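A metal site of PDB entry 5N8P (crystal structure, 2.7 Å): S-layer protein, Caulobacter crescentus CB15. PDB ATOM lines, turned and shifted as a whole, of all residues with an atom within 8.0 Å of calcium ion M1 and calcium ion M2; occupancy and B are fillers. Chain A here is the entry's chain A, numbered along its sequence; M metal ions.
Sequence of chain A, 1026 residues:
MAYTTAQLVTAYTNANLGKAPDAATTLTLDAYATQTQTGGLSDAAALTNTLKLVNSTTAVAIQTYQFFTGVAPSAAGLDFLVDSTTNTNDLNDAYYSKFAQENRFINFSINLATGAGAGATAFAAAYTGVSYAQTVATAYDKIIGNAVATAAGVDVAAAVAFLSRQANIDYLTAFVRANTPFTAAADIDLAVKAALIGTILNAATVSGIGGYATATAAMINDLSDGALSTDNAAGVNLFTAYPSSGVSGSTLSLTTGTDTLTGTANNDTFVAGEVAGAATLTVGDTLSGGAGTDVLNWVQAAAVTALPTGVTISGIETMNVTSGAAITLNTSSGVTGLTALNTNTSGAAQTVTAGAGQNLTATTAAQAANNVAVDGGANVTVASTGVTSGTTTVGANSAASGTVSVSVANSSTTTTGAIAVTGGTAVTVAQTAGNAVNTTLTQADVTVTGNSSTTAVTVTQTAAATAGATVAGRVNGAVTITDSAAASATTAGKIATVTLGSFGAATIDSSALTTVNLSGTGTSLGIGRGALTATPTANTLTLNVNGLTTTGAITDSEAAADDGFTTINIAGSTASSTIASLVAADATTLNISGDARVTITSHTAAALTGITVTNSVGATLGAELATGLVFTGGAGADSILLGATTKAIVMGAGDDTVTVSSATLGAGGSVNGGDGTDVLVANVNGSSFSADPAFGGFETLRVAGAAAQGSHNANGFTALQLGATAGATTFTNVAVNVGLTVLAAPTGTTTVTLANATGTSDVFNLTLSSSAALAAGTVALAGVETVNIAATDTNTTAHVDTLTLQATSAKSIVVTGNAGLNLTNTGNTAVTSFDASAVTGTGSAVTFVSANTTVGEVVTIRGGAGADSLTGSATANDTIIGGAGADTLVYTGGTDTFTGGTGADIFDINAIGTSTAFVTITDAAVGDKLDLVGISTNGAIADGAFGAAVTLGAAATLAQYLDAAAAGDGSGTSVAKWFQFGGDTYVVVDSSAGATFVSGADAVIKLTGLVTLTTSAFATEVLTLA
The backbone carbonyl oxygen (O) of Ser 488 lies within hydrogen-bond range of the backbone NH (N) of Leu 532.
N of Gly 564 sits close to OD2 of Asp 586.
Three residues have an atom within 4 Å of calcium ion M1: Ala 559, Asp 562 and Asp 586.
The nearest printed residue that does not touch calcium ion M1 is Ala 560 (4.2 Å).
Two residues have an atom within 4 Å of calcium ion M2: Leu 532 and Asp 562.
Along chain A the residues within 4 Å of calcium ion M2 span positions 532 to 562.
The nearest printed residue that does not touch calcium ion M2 is Thr 533 (4.1 Å).
Calcium ion M1 is bound by the backbone carbonyl oxygen (O) of Asp 562 (2.5 Å), the side-chain carboxylate (OD2) of Asp 586 (2.5 Å), the backbone carbonyl oxygen (O) of Ala 559 (2.7 Å) and the side-chain carboxylate (OD1) of Asp 586 (2.8 Å).
Calcium ion M2 is bound by O of Leu 532 (2.3 Å), OD2 of Asp 562 (2.4 Å) and OD1 of Asp 562 (2.7 Å).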
ATOM      1  N   SER A 488      12.741  14.785  -2.624  1.00  0.00           N
ATOM      2  CA  SER A 488      11.282  14.555  -2.710  1.00  0.00           C
ATOM      3  C   SER A 488      10.446  15.763  -2.281  1.00  0.00           C
ATOM      4  O   SER A 488      10.841  16.519  -1.377  1.00  0.00           O
ATOM      5  CB  SER A 488      10.887  13.315  -1.887  1.00  0.00           C
ATOM      6  OG  SER A 488       9.520  13.354  -1.472  1.00  0.00           O
ATOM      7  N   ALA A 489       9.297  15.915  -2.934  1.00  0.00           N
ATOM      8  CA  ALA A 489       8.309  16.899  -2.541  1.00  0.00           C
ATOM      9  C   ALA A 489       7.403  16.393  -1.399  1.00  0.00           C
ATOM     10  O   ALA A 489       6.874  17.200  -0.638  1.00  0.00           O
ATOM     11  CB  ALA A 489       7.493  17.366  -3.727  1.00  0.00           C
ATOM     12  N   ARG A 529      17.060  21.545   4.698  1.00  0.00           N
ATOM     13  CA  ARG A 529      15.997  20.582   4.983  1.00  0.00           C
ATOM     14  C   ARG A 529      15.473  20.056   3.624  1.00  0.00           C
ATOM     15  O   ARG A 529      15.707  20.668   2.553  1.00  0.00           O
ATOM     16  CB  ARG A 529      14.908  21.254   5.835  1.00  0.00           C
ATOM     17  CG  ARG A 529      15.476  22.205   6.891  1.00  0.00           C
ATOM     18  CD  ARG A 529      14.396  22.969   7.649  1.00  0.00           C
ATOM     19  NE  ARG A 529      13.873  22.161   8.758  1.00  0.00           N
ATOM     20  CZ  ARG A 529      12.760  22.449   9.443  1.00  0.00           C
ATOM     21  NH1 ARG A 529      12.063  23.545   9.173  1.00  0.00           N
ATOM     22  NH2 ARG A 529      12.376  21.661  10.446  1.00  0.00           N
ATOM     23  N   GLY A 530      14.819  18.908   3.632  1.00  0.00           N
ATOM     24  CA  GLY A 530      14.351  18.335   2.371  1.00  0.00           C
ATOM     25  C   GLY A 530      13.463  19.303   1.599  1.00  0.00           C
ATOM     26  O   GLY A 530      12.768  20.162   2.210  1.00  0.00           O
ATOM     27  N   ALA A 531      13.463  19.170   0.271  1.00  0.00           N
ATOM     28  CA  ALA A 531      12.675  20.065  -0.589  1.00  0.00           C
ATOM     29  C   ALA A 531      11.143  19.794  -0.570  1.00  0.00           C
ATOM     30  O   ALA A 531      10.422  20.144  -1.518  1.00  0.00           O
ATOM     31  CB  ALA A 531      13.262  20.130  -1.999  1.00  0.00           C
ATOM     32  N   LEU A 532      10.659  19.197   0.536  1.00  0.00           N
ATOM     33  CA  LEU A 532       9.242  19.132   0.899  1.00  0.00           C
ATOM     34  C   LEU A 532       8.507  20.417   0.589  1.00  0.00           C
ATOM     35  O   LEU A 532       8.977  21.500   0.960  1.00  0.00           O
ATOM     36  CB  LEU A 532       9.103  18.834   2.382  1.00  0.00           C
ATOM     37  CG  LEU A 532       8.636  17.467   2.847  1.00  0.00           C
ATOM     38  CD1 LEU A 532       9.510  16.377   2.236  1.00  0.00           C
ATOM     39  CD2 LEU A 532       8.604  17.391   4.377  1.00  0.00           C
ATOM     40  N   THR A 533       7.366  20.324  -0.097  1.00  0.00           N
ATOM     41  CA  THR A 533       6.600  21.524  -0.473  1.00  0.00           C
ATOM     42  C   THR A 533       5.652  21.956   0.639  1.00  0.00           C
ATOM     43  O   THR A 533       5.460  23.155   0.830  1.00  0.00           O
ATOM     44  CB  THR A 533       5.851  21.389  -1.816  1.00  0.00           C
ATOM     45  OG1 THR A 533       5.048  20.198  -1.782  1.00  0.00           O
ATOM     46  CG2 THR A 533       6.829  21.376  -3.023  1.00  0.00           C
ATOM     47  N   ALA A 534       5.088  20.985   1.370  1.00  0.00           N
ATOM     48  CA  ALA A 534       4.337  21.192   2.625  1.00  0.00           C
ATOM     49  C   ALA A 534       5.056  22.152   3.616  1.00  0.00           C
ATOM     50  O   ALA A 534       6.274  22.052   3.839  1.00  0.00           O
ATOM     51  CB  ALA A 534       4.049  19.857   3.294  1.00  0.00           C
ATOM     52  N   THR A 535       4.288  23.089   4.183  1.00  0.00           N
ATOM     53  CA  THR A 535       4.808  24.018   5.193  1.00  0.00           C
ATOM     54  C   THR A 535       5.037  23.314   6.544  1.00  0.00           C
ATOM     55  O   THR A 535       4.080  22.809   7.157  1.00  0.00           O
ATOM     56  CB  THR A 535       3.953  25.318   5.289  1.00  0.00           C
ATOM     57  OG1 THR A 535       4.279  26.166   4.182  1.00  0.00           O
ATOM     58  CG2 THR A 535       4.236  26.099   6.583  1.00  0.00           C
ATOM     59  N   PRO A 536       6.304  23.286   7.002  1.00  0.00           N
ATOM     60  CA  PRO A 536       6.702  22.492   8.173  1.00  0.00           C
ATOM     61  C   PRO A 536       6.169  23.091   9.447  1.00  0.00           C
ATOM     62  O   PRO A 536       6.098  24.313   9.577  1.00  0.00           O
ATOM     63  CB  PRO A 536       8.234  22.527   8.123  1.00  0.00           C
ATOM     64  CG  PRO A 536       8.627  23.218   6.848  1.00  0.00           C
ATOM     65  CD  PRO A 536       7.441  24.071   6.483  1.00  0.00           C
ATOM     66  N   GLU A 558      18.169  26.463   4.291  1.00  0.00           N
ATOM     67  CA  GLU A 558      16.734  26.356   3.991  1.00  0.00           C
ATOM     68  C   GLU A 558      15.980  27.666   4.241  1.00  0.00           C
ATOM     69  O   GLU A 558      15.066  27.987   3.496  1.00  0.00           O
ATOM     70  CB  GLU A 558      16.053  25.131   4.659  1.00  0.00           C
ATOM     71  CG  GLU A 558      14.866  24.471   3.894  1.00  0.00           C
ATOM     72  CD  GLU A 558      15.153  23.864   2.488  1.00  0.00           C
ATOM     73  OE1 GLU A 558      16.316  23.690   2.042  1.00  0.00           O
ATOM     74  OE2 GLU A 558      14.185  23.544   1.747  1.00  0.00           O
ATOM     75  N   ALA A 559      16.398  28.454   5.237  1.00  0.00           N
ATOM     76  CA  ALA A 559      15.671  29.667   5.655  1.00  0.00           C
ATOM     77  C   ALA A 559      15.528  30.755   4.564  1.00  0.00           C
ATOM     78  O   ALA A 559      14.426  31.353   4.401  1.00  0.00           O
ATOM     79  CB  ALA A 559      16.293  30.240   6.928  1.00  0.00           C
ATOM     80  N   ALA A 560      16.637  30.957   3.829  1.00  0.00           N
ATOM     81  CA  ALA A 560      16.762  31.957   2.761  1.00  0.00           C
ATOM     82  C   ALA A 560      15.560  32.005   1.792  1.00  0.00           C
ATOM     83  O   ALA A 560      14.752  32.921   1.848  1.00  0.00           O
ATOM     84  CB  ALA A 560      18.068  31.757   2.012  1.00  0.00           C
ATOM     85  N   ALA A 561      15.420  30.966   0.956  1.00  0.00           N
ATOM     86  CA  ALA A 561      14.333  30.875  -0.028  1.00  0.00           C
ATOM     87  C   ALA A 561      13.171  29.919   0.338  1.00  0.00           C
ATOM     88  O   ALA A 561      12.199  29.815  -0.430  1.00  0.00           O
ATOM     89  CB  ALA A 561      14.885  30.556  -1.420  1.00  0.00           C
ATOM     90  N   ASP A 562      13.249  29.259   1.502  1.00  0.00           N
ATOM     91  CA  ASP A 562      12.281  28.216   1.885  1.00  0.00           C
ATOM     92  C   ASP A 562      11.979  28.366   3.367  1.00  0.00           C
ATOM     93  O   ASP A 562      12.166  29.454   3.909  1.00  0.00           O
ATOM     94  CB  ASP A 562      12.847  26.824   1.527  1.00  0.00           C
ATOM     95  CG  ASP A 562      11.759  25.795   1.168  1.00  0.00           C
ATOM     96  OD1 ASP A 562      11.763  25.272   0.019  1.00  0.00           O
ATOM     97  OD2 ASP A 562      10.903  25.464   2.011  1.00  0.00           O
ATOM     98  N   ASP A 563      11.548  27.284   4.019  1.00  0.00           N
ATOM     99  CA  ASP A 563      11.109  27.340   5.415  1.00  0.00           C
ATOM    100  C   ASP A 563      12.118  26.766   6.410  1.00  0.00           C
ATOM    101  O   ASP A 563      12.151  25.553   6.677  1.00  0.00           O
ATOM    102  CB  ASP A 563       9.725  26.688   5.598  1.00  0.00           C
ATOM    103  CG  ASP A 563       8.664  27.214   4.606  1.00  0.00           C
ATOM    104  OD1 ASP A 563       8.884  28.252   3.901  1.00  0.00           O
ATOM    105  OD2 ASP A 563       7.588  26.568   4.529  1.00  0.00           O
ATOM    106  N   GLY A 564      12.935  27.670   6.966  1.00  0.00           N
ATOM    107  CA  GLY A 564      13.985  27.326   7.930  1.00  0.00           C
ATOM    108  C   GLY A 564      13.483  27.016   9.329  1.00  0.00           C
ATOM    109  O   GLY A 564      12.290  26.715   9.553  1.00  0.00           O
ATOM    110  N   PHE A 565      14.418  27.044  10.281  1.00  0.00           N
ATOM    111  CA  PHE A 565      14.096  26.904  11.695  1.00  0.00           C
ATOM    112  C   PHE A 565      13.747  28.276  12.285  1.00  0.00           C
ATOM    113  O   PHE A 565      14.470  29.282  12.039  1.00  0.00           O
ATOM    114  CB  PHE A 565      15.251  26.295  12.465  1.00  0.00           C
ATOM    115  CG  PHE A 565      15.707  24.966  11.945  1.00  0.00           C
ATOM    116  CD1 PHE A 565      16.645  24.889  10.916  1.00  0.00           C
ATOM    117  CD2 PHE A 565      15.197  23.778  12.484  1.00  0.00           C
ATOM    118  CE1 PHE A 565      17.072  23.648  10.441  1.00  0.00           C
ATOM    119  CE2 PHE A 565      15.621  22.550  12.003  1.00  0.00           C
ATOM    120  CZ  PHE A 565      16.541  22.483  10.984  1.00  0.00           C
ATOM    121  N   ALA A 585      18.406  33.071   8.913  1.00  0.00           N
ATOM    122  CA  ALA A 585      17.437  34.091   8.459  1.00  0.00           C
ATOM    123  C   ALA A 585      15.946  33.895   8.806  1.00  0.00           C
ATOM    124  O   ALA A 585      15.182  34.840   8.689  1.00  0.00           O
ATOM    125  CB  ALA A 585      17.615  34.398   6.965  1.00  0.00           C
ATOM    126  N   ASP A 586      15.515  32.711   9.259  1.00  0.00           N
ATOM    127  CA  ASP A 586      14.092  32.516   9.649  1.00  0.00           C
ATOM    128  C   ASP A 586      13.961  32.392  11.179  1.00  0.00           C
ATOM    129  O   ASP A 586      12.894  32.059  11.709  1.00  0.00           O
ATOM    130  CB  ASP A 586      13.408  31.307   8.958  1.00  0.00           C
ATOM    131  CG  ASP A 586      12.913  31.604   7.505  1.00  0.00           C
ATOM    132  OD1 ASP A 586      13.021  32.766   6.999  1.00  0.00           O
ATOM    133  OD2 ASP A 586      12.388  30.654   6.836  1.00  0.00           O
ATOM    134  N   ALA A 587      15.056  32.631  11.874  1.00  0.00           N
ATOM    135  CA  ALA A 587      15.062  32.455  13.314  1.00  0.00           C
ATOM    136  C   ALA A 587      14.423  33.619  14.098  1.00  0.00           C
ATOM    137  O   ALA A 587      14.610  34.808  13.771  1.00  0.00           O
ATOM    138  CB  ALA A 587      16.462  32.145  13.831  1.00  0.00           C
HETATM  139 CA    CA M   1      11.810  31.817   4.656  1.00  0.00          CA
HETATM  140 CA    CA M   2       9.831  23.649   0.860  1.00  0.00          CA
HETATM  141 CA    CA M   3      15.662  22.304   0.286  1.00  0.00          CA
